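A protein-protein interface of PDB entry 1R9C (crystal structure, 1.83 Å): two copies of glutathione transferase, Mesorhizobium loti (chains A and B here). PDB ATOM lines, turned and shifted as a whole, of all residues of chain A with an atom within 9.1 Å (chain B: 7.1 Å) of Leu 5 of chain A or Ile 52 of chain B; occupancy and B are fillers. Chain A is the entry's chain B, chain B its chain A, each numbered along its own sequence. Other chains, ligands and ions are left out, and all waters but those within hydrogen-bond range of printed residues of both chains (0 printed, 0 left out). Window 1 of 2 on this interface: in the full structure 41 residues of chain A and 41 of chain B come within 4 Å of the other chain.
The backbone carbonyl oxygen (O) of Ala 71 of chain A lies within hydrogen-bond range of the backbone NH (N) of Ser 6 of chain B, at 2.8 Å. The backbone NH (N) of Ala 71 of chain A sits at hydrogen-bond distance from the backbone carbonyl oxygen (O) of His 7 of chain B, at 2.9 Å. The backbone carbonyl oxygen of Ala 71 of chain B sits at hydrogen-bond distance from the backbone NH of Ser 6 of chain A (2.7 Å). The backbone carbonyl oxygen (O) of His 7 of chain A sits at hydrogen-bond distance from the backbone NH (N) of Ala 71 of chain B. OE1 of Glu 3 of chain A lies within salt-bridge range of NZ of Lys 73 of chain B, 3.0 Å away. N of Lys 73 of chain B lies within hydrogen-bond range of O of Gly 4 of chain A.
The side-chain hydroxyl of Ser 6 of chain B sits at hydrogen-bond distance from a ring nitrogen (ND1) of His 7 of chain B, at 2.9 Å. The backbone NH (N) of Met 8 of chain B is in hydrogen-bond range of the backbone carbonyl oxygen (O) of Trp 53 of chain B. OG of Ser 6 of chain A sits at hydrogen-bond distance from ND1 of His 7 of chain A, at 3.0 Å. The backbone NH (N) of Met 8 of chain A sits at hydrogen-bond distance from the backbone carbonyl oxygen (O) of Trp 53 of chain A, at 3.1 Å.
CG2 of Ile 2 of chain A touches CD2 of Phe 72 of chain B, 3.95 Å away. Ile 2 of chain A touches Lys 73 of chain B (CA to O, 3.7 Å). Gly 4 of chain A touches Ile 52 of chain B (C to CD1, 3.95 Å). O of Gly 4 of chain A touches CA of Phe 72 of chain B (3.5 Å). CD1 of Leu 5 of chain A touches O of Ala 71 of chain B (3.6 Å). Ile 70 of chain A touches Leu 5 of chain B. His 7 of chain B touches Ile 70 of chain A. Ile 70 of chain A touches Met 8 of chain B (CD1 to CB, 3.6 Å). Leu 124 of chain A touches Leu 48 of chain B.
Of chain B, only Ile 52 (3.7 Å), Ile 70 (3.9 Å) and Ala 71 (3.6 Å) come within 4 Å of Leu 5 of chain A. Of chain A, only Gly 4 (3.95 Å) and Leu 5 (3.7 Å) come within 4 Å of Ile 52 of chain B. No residue of chain A comes within 4 Å of Gly 50 of chain B. No residue of chain A comes within 4 Å of Asp 51 of chain B. Of the printed residues of chain A, Ser 6 of chain B touches Ala 71 and Phe 72. Of the printed residues of chain B, Phe 72 of chain A touches Ser 6. Of the printed residues of chain A, Phe 72 of chain B touches Ile 2 (3.95 Å), Gly 4 (3.5 Å) and Ser 6 (3.7 Å). Printed residues of chain B within 4 Å of Leu 124 of chain A: Leu 48 (3.8 Å) and Trp 53 (3.6 Å). Asp 51 of chain A touches none of the printed residues of chain B. Trp 53 of chain A touches none of the printed residues of chain B. The nearest residue of chain A that does not touch Ile 52 of chain B is Ile 2 of chain A (5.5 Å). The nearest printed residue of chain B that does not touch Ile 52 of chain A is Ser 6 of chain B (6.6 Å).
Of the 18 printed residues of chain B, 12 touch a printed residue of chain A. Hydrophobic or aromatic side chains of chain B within 4 Å of the printed part of chain A: Leu 5, His 7, Met 8, Leu 48, Ile 49, Ile 52, Trp 53, Ile 70, Ala 71 and Phe 72. Printed residues of chain A that touch a printed residue of chain B: Ile 2, Glu 3, Gly 4, Leu 5, Ser 6, His 7, Met 8, Ile 52, Ile 70, Ala 71, Phe 72 and Leu 124. Hydrophobic or aromatic side chains of chain A that line the printed part of chain B: Ile 2, Leu 5, His 7, Met 8, Ile 52, Ile 70, Ala 71 and Leu 124. Among the printed residues, Asp or Glu carboxylates within 4 Å of a Lys or Arg side-chain nitrogen of the other chain: Glu 3 of chain A with Lys 73 of chain B.
Leu 5 of chain A touches Ile 52 of chain B, and with the chains exchanged Ile 52 of chain A touches Leu 5 of chain B. Ser 6 of chain A touches Phe 72 of chain B, and with the chains exchanged Phe 72 of chain A touches Ser 6 of chain B. His 7 of chain A touches Ile 70 of chain B, and with the chains exchanged Ile 70 of chain A touches His 7 of chain B. Met 8 of chain A touches Ile 70 of chain B, and with the chains exchanged Ile 70 of chain A touches Met 8 of chain B.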
ATOM      1  N   ILE A   2     -16.276  36.868  -1.724  1.00  0.00           N
ATOM      2  CA  ILE A   2     -17.138  36.289  -2.758  1.00  0.00           C
ATOM      3  C   ILE A   2     -17.954  35.170  -2.130  1.00  0.00           C
ATOM      4  O   ILE A   2     -17.395  34.246  -1.499  1.00  0.00           O
ATOM      5  CB  ILE A   2     -16.314  35.738  -3.959  1.00  0.00           C
ATOM      6  CG1 ILE A   2     -15.452  36.839  -4.582  1.00  0.00           C
ATOM      7  CG2 ILE A   2     -17.259  35.160  -5.011  1.00  0.00           C
ATOM      8  CD1 ILE A   2     -16.238  37.976  -5.302  1.00  0.00           C
ATOM      9  N   GLU A   3     -19.276  35.254  -2.277  1.00  0.00           N
ATOM     10  CA  GLU A   3     -20.160  34.311  -1.591  1.00  0.00           C
ATOM     11  C   GLU A   3     -20.410  33.073  -2.455  1.00  0.00           C
ATOM     12  O   GLU A   3     -20.751  32.003  -1.941  1.00  0.00           O
ATOM     13  CB  GLU A   3     -21.498  34.969  -1.245  1.00  0.00           C
ATOM     14  CG  GLU A   3     -21.383  36.126  -0.282  1.00  0.00           C
ATOM     15  CD  GLU A   3     -22.708  36.833  -0.028  1.00  0.00           C
ATOM     16  OE1 GLU A   3     -23.767  36.376  -0.529  1.00  0.00           O
ATOM     17  OE2 GLU A   3     -22.677  37.834   0.707  1.00  0.00           O
ATOM     18  N   GLY A   4     -20.255  33.243  -3.758  1.00  0.00           N
ATOM     19  CA  GLY A   4     -20.498  32.186  -4.726  1.00  0.00           C
ATOM     20  C   GLY A   4     -20.852  32.783  -6.080  1.00  0.00           C
ATOM     21  O   GLY A   4     -20.699  33.981  -6.292  1.00  0.00           O
ATOM     22  N   LEU A   5     -21.355  31.946  -6.981  1.00  0.00           N
ATOM     23  CA  LEU A   5     -21.803  32.409  -8.282  1.00  0.00           C
ATOM     24  C   LEU A   5     -23.145  33.107  -8.104  1.00  0.00           C
ATOM     25  O   LEU A   5     -23.982  32.619  -7.369  1.00  0.00           O
ATOM     26  CB  LEU A   5     -21.996  31.210  -9.232  1.00  0.00           C
ATOM     27  CG  LEU A   5     -22.210  31.563 -10.708  1.00  0.00           C
ATOM     28  CD1 LEU A   5     -20.921  31.958 -11.297  1.00  0.00           C
ATOM     29  CD2 LEU A   5     -22.707  30.273 -11.415  1.00  0.00           C
ATOM     30  N   SER A   6     -23.343  34.242  -8.767  1.00  0.00           N
ATOM     31  CA  SER A   6     -24.658  34.868  -8.786  1.00  0.00           C
ATOM     32  C   SER A   6     -25.419  34.348  -9.983  1.00  0.00           C
ATOM     33  O   SER A   6     -26.502  33.775  -9.821  1.00  0.00           O
ATOM     34  CB  SER A   6     -24.557  36.395  -8.846  1.00  0.00           C
ATOM     35  OG  SER A   6     -25.858  36.934  -8.933  1.00  0.00           O
ATOM     36  N   HIS A   7     -24.881  34.571 -11.189  1.00  0.00           N
ATOM     37  CA  HIS A   7     -25.575  34.171 -12.429  1.00  0.00           C
ATOM     38  C   HIS A   7     -24.614  34.175 -13.605  1.00  0.00           C
ATOM     39  O   HIS A   7     -23.490  34.674 -13.500  1.00  0.00           O
ATOM     40  CB  HIS A   7     -26.807  35.100 -12.749  1.00  0.00           C
ATOM     41  CG  HIS A   7     -26.487  36.569 -12.914  1.00  0.00           C
ATOM     42  ND1 HIS A   7     -26.441  37.441 -11.853  1.00  0.00           N
ATOM     43  CD2 HIS A   7     -26.291  37.331 -14.026  1.00  0.00           C
ATOM     44  CE1 HIS A   7     -26.218  38.675 -12.294  1.00  0.00           C
ATOM     45  NE2 HIS A   7     -26.124  38.642 -13.612  1.00  0.00           N
ATOM     46  N   MET A   8     -25.047  33.594 -14.723  1.00  0.00           N
ATOM     47  CA  MET A   8     -24.323  33.691 -15.986  1.00  0.00           C
ATOM     48  C   MET A   8     -25.314  34.117 -17.046  1.00  0.00           C
ATOM     49  O   MET A   8     -26.470  33.617 -17.089  1.00  0.00           O
ATOM     50  CB  MET A   8     -23.684  32.335 -16.365  1.00  0.00           C
ATOM     51  CG  MET A   8     -24.647  31.166 -16.412  1.00  0.00           C
ATOM     52  SD  MET A   8     -23.869  29.518 -16.809  1.00  0.00           S
ATOM     53  CE  MET A   8     -22.774  29.330 -15.388  1.00  0.00           C
ATOM     54  N   THR A   9     -24.884  35.060 -17.877  1.00  0.00           N
ATOM     55  CA  THR A   9     -25.767  35.709 -18.843  1.00  0.00           C
ATOM     56  C   THR A   9     -25.193  35.486 -20.234  1.00  0.00           C
ATOM     57  O   THR A   9     -23.972  35.715 -20.447  1.00  0.00           O
ATOM     58  CB  THR A   9     -25.823  37.219 -18.543  1.00  0.00           C
ATOM     59  OG1 THR A   9     -26.516  37.431 -17.304  1.00  0.00           O
ATOM     60  CG2 THR A   9     -26.680  37.976 -19.563  1.00  0.00           C
ATOM     61  N   PHE A  10     -26.071  35.063 -21.159  1.00  0.00           N
ATOM     62  CA  PHE A  10     -25.729  34.850 -22.571  1.00  0.00           C
ATOM     63  C   PHE A  10     -26.588  35.714 -23.480  1.00  0.00           C
ATOM     64  O   PHE A  10     -27.819  35.833 -23.296  1.00  0.00           O
ATOM     65  CB  PHE A  10     -25.903  33.358 -22.952  1.00  0.00           C
ATOM     66  CG  PHE A  10     -25.096  32.438 -22.096  1.00  0.00           C
ATOM     67  CD1 PHE A  10     -25.695  31.743 -21.054  1.00  0.00           C
ATOM     68  CD2 PHE A  10     -23.710  32.355 -22.270  1.00  0.00           C
ATOM     69  CE1 PHE A  10     -24.934  30.942 -20.223  1.00  0.00           C
ATOM     70  CE2 PHE A  10     -22.930  31.539 -21.445  1.00  0.00           C
ATOM     71  CZ  PHE A  10     -23.533  30.841 -20.429  1.00  0.00           C
ATOM     72  N   ILE A  49     -30.656  26.212 -13.666  1.00  0.00           N
ATOM     73  CA  ILE A  49     -30.154  24.851 -13.848  1.00  0.00           C
ATOM     74  C   ILE A  49     -29.725  24.381 -12.467  1.00  0.00           C
ATOM     75  O   ILE A  49     -28.596  24.666 -12.024  1.00  0.00           O
ATOM     76  CB  ILE A  49     -28.985  24.845 -14.837  1.00  0.00           C
ATOM     77  CG1 ILE A  49     -29.469  25.361 -16.217  1.00  0.00           C
ATOM     78  CG2 ILE A  49     -28.369  23.416 -14.933  1.00  0.00           C
ATOM     79  CD1 ILE A  49     -28.364  25.744 -17.184  1.00  0.00           C
ATOM     80  N   ASP A  51     -29.363  25.122  -9.041  1.00  0.00           N
ATOM     81  CA  ASP A  51     -29.450  26.395  -8.366  1.00  0.00           C
ATOM     82  C   ASP A  51     -28.656  27.477  -9.089  1.00  0.00           C
ATOM     83  O   ASP A  51     -28.438  28.554  -8.540  1.00  0.00           O
ATOM     84  CB  ASP A  51     -29.098  26.275  -6.886  1.00  0.00           C
ATOM     85  CG  ASP A  51     -27.689  25.787  -6.656  1.00  0.00           C
ATOM     86  OD1 ASP A  51     -26.959  25.560  -7.634  1.00  0.00           O
ATOM     87  OD2 ASP A  51     -27.243  25.599  -5.506  1.00  0.00           O
ATOM     88  N   ILE A  52     -28.310  27.195 -10.340  1.00  0.00           N
ATOM     89  CA  ILE A  52     -27.537  28.128 -11.166  1.00  0.00           C
ATOM     90  C   ILE A  52     -28.528  28.954 -11.956  1.00  0.00           C
ATOM     91  O   ILE A  52     -29.299  28.437 -12.764  1.00  0.00           O
ATOM     92  CB  ILE A  52     -26.551  27.384 -12.119  1.00  0.00           C
ATOM     93  CG1 ILE A  52     -25.527  26.566 -11.301  1.00  0.00           C
ATOM     94  CG2 ILE A  52     -25.815  28.358 -13.022  1.00  0.00           C
ATOM     95  CD1 ILE A  52     -24.963  25.372 -12.062  1.00  0.00           C
ATOM     96  N   TRP A  53     -28.510  30.239 -11.661  1.00  0.00           N
ATOM     97  CA  TRP A  53     -29.280  31.244 -12.353  1.00  0.00           C
ATOM     98  C   TRP A  53     -28.629  31.547 -13.688  1.00  0.00           C
ATOM     99  O   TRP A  53     -27.457  31.956 -13.755  1.00  0.00           O
ATOM    100  CB  TRP A  53     -29.351  32.492 -11.449  1.00  0.00           C
ATOM    101  CG  TRP A  53     -30.027  33.718 -12.020  1.00  0.00           C
ATOM    102  CD1 TRP A  53     -30.741  33.833 -13.208  1.00  0.00           C
ATOM    103  CD2 TRP A  53     -30.056  35.010 -11.416  1.00  0.00           C
ATOM    104  NE1 TRP A  53     -31.211  35.119 -13.349  1.00  0.00           N
ATOM    105  CE2 TRP A  53     -30.789  35.868 -12.276  1.00  0.00           C
ATOM    106  CE3 TRP A  53     -29.533  35.540 -10.218  1.00  0.00           C
ATOM    107  CZ2 TRP A  53     -31.010  37.229 -11.980  1.00  0.00           C
ATOM    108  CZ3 TRP A  53     -29.755  36.892  -9.921  1.00  0.00           C
ATOM    109  CH2 TRP A  53     -30.490  37.715 -10.800  1.00  0.00           C
ATOM    110  N   VAL A  54     -29.378  31.323 -14.766  1.00  0.00           N
ATOM    111  CA  VAL A  54     -28.960  31.713 -16.132  1.00  0.00           C
ATOM    112  C   VAL A  54     -29.911  32.760 -16.710  1.00  0.00           C
ATOM    113  O   VAL A  54     -31.131  32.541 -16.732  1.00  0.00           O
ATOM    114  CB  VAL A  54     -28.969  30.493 -17.108  1.00  0.00           C
ATOM    115  CG1 VAL A  54     -28.470  30.897 -18.528  1.00  0.00           C
ATOM    116  CG2 VAL A  54     -28.126  29.409 -16.571  1.00  0.00           C
ATOM    117  N   ILE A  70     -18.083  27.290 -20.638  1.00  0.00           N
ATOM    118  CA  ILE A  70     -18.655  26.975 -19.338  1.00  0.00           C
ATOM    119  C   ILE A  70     -18.952  25.500 -19.308  1.00  0.00           C
ATOM    120  O   ILE A  70     -19.569  24.974 -20.242  1.00  0.00           O
ATOM    121  CB  ILE A  70     -19.952  27.767 -19.093  1.00  0.00           C
ATOM    122  CG1 ILE A  70     -19.698  29.304 -19.096  1.00  0.00           C
ATOM    123  CG2 ILE A  70     -20.654  27.272 -17.803  1.00  0.00           C
ATOM    124  CD1 ILE A  70     -18.670  29.761 -18.146  1.00  0.00           C
ATOM    125  N   ALA A  71     -18.560  24.848 -18.217  1.00  0.00           N
ATOM    126  CA  ALA A  71     -18.712  23.413 -18.104  1.00  0.00           C
ATOM    127  C   ALA A  71     -19.560  23.018 -16.899  1.00  0.00           C
ATOM    128  O   ALA A  71     -19.393  23.568 -15.789  1.00  0.00           O
ATOM    129  CB  ALA A  71     -17.369  22.748 -18.047  1.00  0.00           C
ATOM    130  N   PHE A  72     -20.477  22.073 -17.155  1.00  0.00           N
ATOM    131  CA  PHE A  72     -21.379  21.560 -16.138  1.00  0.00           C
ATOM    132  C   PHE A  72     -20.998  20.137 -15.810  1.00  0.00           C
ATOM    133  O   PHE A  72     -20.544  19.391 -16.668  1.00  0.00           O
ATOM    134  CB  PHE A  72     -22.837  21.640 -16.616  1.00  0.00           C
ATOM    135  CG  PHE A  72     -23.349  23.049 -16.723  1.00  0.00           C
ATOM    136  CD1 PHE A  72     -23.368  23.697 -17.952  1.00  0.00           C
ATOM    137  CD2 PHE A  72     -23.765  23.731 -15.594  1.00  0.00           C
ATOM    138  CE1 PHE A  72     -23.818  25.023 -18.061  1.00  0.00           C
ATOM    139  CE2 PHE A  72     -24.241  25.047 -15.671  1.00  0.00           C
ATOM    140  CZ  PHE A  72     -24.254  25.701 -16.913  1.00  0.00           C
ATOM    141  N   LEU A 124     -12.185  18.277 -10.147  1.00  0.00           N
ATOM    142  CA  LEU A 124     -10.913  18.966 -10.011  1.00  0.00           C
ATOM    143  C   LEU A 124      -9.900  18.082  -9.344  1.00  0.00           C
ATOM    144  O   LEU A 124      -8.787  17.943  -9.849  1.00  0.00           O
ATOM    145  CB  LEU A 124     -11.099  20.270  -9.225  1.00  0.00           C
ATOM    146  CG  LEU A 124      -9.854  21.083  -8.854  1.00  0.00           C
ATOM    147  CD1 LEU A 124      -9.007  21.462 -10.080  1.00  0.00           C
ATOM    148  CD2 LEU A 124     -10.277  22.311  -8.060  1.00  0.00           C
ATOM    149  N   LEU B   5     -22.111  23.196 -11.400  1.00  0.00           N
ATOM    150  CA  LEU B   5     -21.082  23.720 -12.289  1.00  0.00           C
ATOM    151  C   LEU B   5     -19.790  22.924 -12.082  1.00  0.00           C
ATOM    152  O   LEU B   5     -19.396  22.665 -10.929  1.00  0.00           O
ATOM    153  CB  LEU B   5     -20.836  25.198 -11.968  1.00  0.00           C
ATOM    154  CG  LEU B   5     -19.731  25.973 -12.660  1.00  0.00           C
ATOM    155  CD1 LEU B   5     -20.167  26.361 -14.042  1.00  0.00           C
ATOM    156  CD2 LEU B   5     -19.414  27.200 -11.788  1.00  0.00           C
ATOM    157  N   SER B   6     -19.127  22.558 -13.176  1.00  0.00           N
ATOM    158  CA  SER B   6     -17.816  21.919 -13.107  1.00  0.00           C
ATOM    159  C   SER B   6     -16.733  22.999 -13.065  1.00  0.00           C
ATOM    160  O   SER B   6     -15.981  23.116 -12.077  1.00  0.00           O
ATOM    161  CB  SER B   6     -17.611  20.981 -14.308  1.00  0.00           C
ATOM    162  OG  SER B   6     -16.275  20.476 -14.360  1.00  0.00           O
ATOM    163  N   HIS B   7     -16.640  23.782 -14.139  1.00  0.00           N
ATOM    164  CA  HIS B   7     -15.620  24.821 -14.227  1.00  0.00           C
ATOM    165  C   HIS B   7     -16.018  25.905 -15.237  1.00  0.00           C
ATOM    166  O   HIS B   7     -16.958  25.704 -16.018  1.00  0.00           O
ATOM    167  CB  HIS B   7     -14.228  24.218 -14.578  1.00  0.00           C
ATOM    168  CG  HIS B   7     -14.163  23.441 -15.875  1.00  0.00           C
ATOM    169  ND1 HIS B   7     -14.447  22.094 -15.945  1.00  0.00           N
ATOM    170  CD2 HIS B   7     -13.734  23.792 -17.119  1.00  0.00           C
ATOM    171  CE1 HIS B   7     -14.243  21.663 -17.184  1.00  0.00           C
ATOM    172  NE2 HIS B   7     -13.793  22.669 -17.919  1.00  0.00           N
ATOM    173  N   MET B   8     -15.358  27.061 -15.159  1.00  0.00           N
ATOM    174  CA  MET B   8     -15.390  28.020 -16.241  1.00  0.00           C
ATOM    175  C   MET B   8     -13.963  28.237 -16.744  1.00  0.00           C
ATOM    176  O   MET B   8     -13.012  28.300 -15.960  1.00  0.00           O
ATOM    177  CB  MET B   8     -16.040  29.335 -15.782  1.00  0.00           C
ATOM    178  CG  MET B   8     -15.288  29.983 -14.611  1.00  0.00           C
ATOM    179  SD  MET B   8     -16.092  31.477 -13.933  1.00  0.00           S
ATOM    180  CE  MET B   8     -17.549  30.741 -13.169  1.00  0.00           C
ATOM    181  N   ARG B  29      -7.523  31.382  -5.399  1.00  0.00           N
ATOM    182  CA  ARG B  29      -6.371  30.625  -4.905  1.00  0.00           C
ATOM    183  C   ARG B  29      -5.869  29.745  -6.071  1.00  0.00           C
ATOM    184  O   ARG B  29      -6.629  28.945  -6.628  1.00  0.00           O
ATOM    185  CB  ARG B  29      -6.804  29.750  -3.710  1.00  0.00           C
ATOM    186  CG  ARG B  29      -5.708  28.878  -3.080  1.00  0.00           C
ATOM    187  CD  ARG B  29      -6.214  27.744  -2.155  1.00  0.00           C
ATOM    188  NE  ARG B  29      -5.641  26.438  -2.521  1.00  0.00           N
ATOM    189  CZ  ARG B  29      -4.347  26.106  -2.424  1.00  0.00           C
ATOM    190  NH1 ARG B  29      -3.449  26.962  -1.938  1.00  0.00           N
ATOM    191  NH2 ARG B  29      -3.947  24.898  -2.815  1.00  0.00           N
ATOM    192  N   PHE B  47      -7.662  27.751 -10.707  1.00  0.00           N
ATOM    193  CA  PHE B  47      -7.888  28.480  -9.481  1.00  0.00           C
ATOM    194  C   PHE B  47      -9.175  28.040  -8.835  1.00  0.00           C
ATOM    195  O   PHE B  47     -10.103  27.557  -9.515  1.00  0.00           O
ATOM    196  CB  PHE B  47      -8.020  29.987  -9.766  1.00  0.00           C
ATOM    197  CG  PHE B  47      -6.758  30.640 -10.255  1.00  0.00           C
ATOM    198  CD1 PHE B  47      -6.426  30.625 -11.622  1.00  0.00           C
ATOM    199  CD2 PHE B  47      -5.935  31.314  -9.378  1.00  0.00           C
ATOM    200  CE1 PHE B  47      -5.283  31.247 -12.078  1.00  0.00           C
ATOM    201  CE2 PHE B  47      -4.751  31.941  -9.841  1.00  0.00           C
ATOM    202  CZ  PHE B  47      -4.436  31.898 -11.188  1.00  0.00           C
ATOM    203  N   LEU B  48      -9.240  28.250  -7.516  1.00  0.00           N
ATOM    204  CA  LEU B  48     -10.500  28.139  -6.795  1.00  0.00           C
ATOM    205  C   LEU B  48     -10.915  29.513  -6.246  1.00  0.00           C
ATOM    206  O   LEU B  48     -10.098  30.274  -5.675  1.00  0.00           O
ATOM    207  CB  LEU B  48     -10.410  27.126  -5.647  1.00  0.00           C
ATOM    208  CG  LEU B  48     -10.488  25.616  -5.906  1.00  0.00           C
ATOM    209  CD1 LEU B  48     -10.178  24.792  -4.646  1.00  0.00           C
ATOM    210  CD2 LEU B  48     -11.893  25.272  -6.414  1.00  0.00           C
ATOM    211  N   ILE B  49     -12.188  29.824  -6.461  1.00  0.00           N
ATOM    212  CA  ILE B  49     -12.845  30.946  -5.801  1.00  0.00           C
ATOM    213  C   ILE B  49     -13.908  30.276  -4.937  1.00  0.00           C
ATOM    214  O   ILE B  49     -14.953  29.916  -5.434  1.00  0.00           O
ATOM    215  CB  ILE B  49     -13.485  31.902  -6.828  1.00  0.00           C
ATOM    216  CG1 ILE B  49     -12.395  32.542  -7.710  1.00  0.00           C
ATOM    217  CG2 ILE B  49     -14.240  33.040  -6.066  1.00  0.00           C
ATOM    218  CD1 ILE B  49     -12.872  33.152  -8.985  1.00  0.00           C
ATOM    219  N   GLY B  50     -13.597  30.054  -3.660  1.00  0.00           N
ATOM    220  CA  GLY B  50     -14.434  29.233  -2.808  1.00  0.00           C
ATOM    221  C   GLY B  50     -14.365  27.806  -3.352  1.00  0.00           C
ATOM    222  O   GLY B  50     -13.296  27.188  -3.402  1.00  0.00           O
ATOM    223  N   ASP B  51     -15.497  27.294  -3.806  1.00  0.00           N
ATOM    224  CA  ASP B  51     -15.499  25.976  -4.434  1.00  0.00           C
ATOM    225  C   ASP B  51     -15.653  26.082  -5.972  1.00  0.00           C
ATOM    226  O   ASP B  51     -15.877  25.075  -6.641  1.00  0.00           O
ATOM    227  CB  ASP B  51     -16.658  25.165  -3.860  1.00  0.00           C
ATOM    228  CG  ASP B  51     -17.985  25.843  -4.092  1.00  0.00           C
ATOM    229  OD1 ASP B  51     -18.021  26.822  -4.862  1.00  0.00           O
ATOM    230  OD2 ASP B  51     -19.058  25.465  -3.582  1.00  0.00           O
ATOM    231  N   ILE B  52     -15.516  27.274  -6.528  1.00  0.00           N
ATOM    232  CA  ILE B  52     -15.655  27.425  -7.984  1.00  0.00           C
ATOM    233  C   ILE B  52     -14.303  27.243  -8.679  1.00  0.00           C
ATOM    234  O   ILE B  52     -13.336  27.927  -8.366  1.00  0.00           O
ATOM    235  CB  ILE B  52     -16.270  28.793  -8.313  1.00  0.00           C
ATOM    236  CG1 ILE B  52     -17.645  28.914  -7.683  1.00  0.00           C
ATOM    237  CG2 ILE B  52     -16.344  29.042  -9.861  1.00  0.00           C
ATOM    238  CD1 ILE B  52     -18.094  30.370  -7.555  1.00  0.00           C
ATOM    239  N   TRP B  53     -14.255  26.303  -9.624  1.00  0.00           N
ATOM    240  CA  TRP B  53     -13.063  26.035 -10.422  1.00  0.00           C
ATOM    241  C   TRP B  53     -13.044  26.964 -11.629  1.00  0.00           C
ATOM    242  O   TRP B  53     -13.967  26.921 -12.461  1.00  0.00           O
ATOM    243  CB  TRP B  53     -13.147  24.588 -10.865  1.00  0.00           C
ATOM    244  CG  TRP B  53     -12.043  24.006 -11.698  1.00  0.00           C
ATOM    245  CD1 TRP B  53     -10.834  24.554 -12.031  1.00  0.00           C
ATOM    246  CD2 TRP B  53     -12.066  22.707 -12.286  1.00  0.00           C
ATOM    247  NE1 TRP B  53     -10.118  23.673 -12.809  1.00  0.00           N
ATOM    248  CE2 TRP B  53     -10.842  22.525 -12.968  1.00  0.00           C
ATOM    249  CE3 TRP B  53     -13.006  21.667 -12.301  1.00  0.00           C
ATOM    250  CZ2 TRP B  53     -10.529  21.342 -13.655  1.00  0.00           C
ATOM    251  CZ3 TRP B  53     -12.688  20.482 -12.972  1.00  0.00           C
ATOM    252  CH2 TRP B  53     -11.468  20.338 -13.642  1.00  0.00           C
ATOM    253  N   VAL B  54     -12.010  27.803 -11.698  1.00  0.00           N
ATOM    254  CA  VAL B  54     -11.738  28.613 -12.858  1.00  0.00           C
ATOM    255  C   VAL B  54     -10.451  28.117 -13.484  1.00  0.00           C
ATOM    256  O   VAL B  54      -9.438  27.963 -12.788  1.00  0.00           O
ATOM    257  CB  VAL B  54     -11.505  30.107 -12.468  1.00  0.00           C
ATOM    258  CG1 VAL B  54     -11.123  30.939 -13.715  1.00  0.00           C
ATOM    259  CG2 VAL B  54     -12.712  30.629 -11.765  1.00  0.00           C
ATOM    260  N   ALA B  55     -10.479  27.889 -14.787  1.00  0.00           N
ATOM    261  CA  ALA B  55      -9.268  27.519 -15.523  1.00  0.00           C
ATOM    262  C   ALA B  55      -8.920  28.650 -16.481  1.00  0.00           C
ATOM    263  O   ALA B  55      -9.797  29.191 -17.141  1.00  0.00           O
ATOM    264  CB  ALA B  55      -9.485  26.218 -16.307  1.00  0.00           C
ATOM    265  N   ILE B  70     -20.249  36.774 -16.646  1.00  0.00           N
ATOM    266  CA  ILE B  70     -20.376  35.876 -15.504  1.00  0.00           C
ATOM    267  C   ILE B  70     -20.407  36.737 -14.255  1.00  0.00           C
ATOM    268  O   ILE B  70     -19.538  37.610 -14.079  1.00  0.00           O
ATOM    269  CB  ILE B  70     -19.169  34.884 -15.441  1.00  0.00           C
ATOM    270  CG1 ILE B  70     -19.088  33.974 -16.677  1.00  0.00           C
ATOM    271  CG2 ILE B  70     -19.194  34.051 -14.153  1.00  0.00           C
ATOM    272  CD1 ILE B  70     -20.352  33.140 -16.966  1.00  0.00           C
ATOM    273  N   ALA B  71     -21.354  36.458 -13.369  1.00  0.00           N
ATOM    274  CA  ALA B  71     -21.597  37.292 -12.190  1.00  0.00           C
ATOM    275  C   ALA B  71     -21.386  36.507 -10.909  1.00  0.00           C
ATOM    276  O   ALA B  71     -21.909  35.403 -10.757  1.00  0.00           O
ATOM    277  CB  ALA B  71     -23.030  37.919 -12.218  1.00  0.00           C
ATOM    278  N   PHE B  72     -20.586  37.081 -10.014  1.00  0.00           N
ATOM    279  CA  PHE B  72     -20.355  36.534  -8.673  1.00  0.00           C
ATOM    280  C   PHE B  72     -21.135  37.297  -7.612  1.00  0.00           C
ATOM    281  O   PHE B  72     -21.402  38.491  -7.736  1.00  0.00           O
ATOM    282  CB  PHE B  72     -18.845  36.561  -8.362  1.00  0.00           C
ATOM    283  CG  PHE B  72     -18.055  35.611  -9.224  1.00  0.00           C
ATOM    284  CD1 PHE B  72     -17.567  36.017 -10.461  1.00  0.00           C
ATOM    285  CD2 PHE B  72     -17.850  34.298  -8.825  1.00  0.00           C
ATOM    286  CE1 PHE B  72     -16.854  35.107 -11.272  1.00  0.00           C
ATOM    287  CE2 PHE B  72     -17.112  33.390  -9.633  1.00  0.00           C
ATOM    288  CZ  PHE B  72     -16.635  33.816 -10.853  1.00  0.00           C
ATOM    289  N   LYS B  73     -21.482  36.615  -6.534  1.00  0.00           N
ATOM    290  CA  LYS B  73     -22.295  37.225  -5.475  1.00  0.00           C
ATOM    291  C   LYS B  73     -21.440  37.852  -4.375  1.00  0.00           C
ATOM    292  O   LYS B  73     -20.499  37.234  -3.877  1.00  0.00           O
ATOM    293  CB  LYS B  73     -23.217  36.153  -4.840  1.00  0.00           C
ATOM    294  CG  LYS B  73     -24.112  36.638  -3.666  1.00  0.00           C
ATOM    295  CD  LYS B  73     -25.217  37.647  -4.127  1.00  0.00           C
ATOM    296  CE  LYS B  73     -26.181  38.000  -2.972  1.00  0.00           C
ATOM    297  NZ  LYS B  73     -25.460  38.594  -1.756  1.00  0.00           N
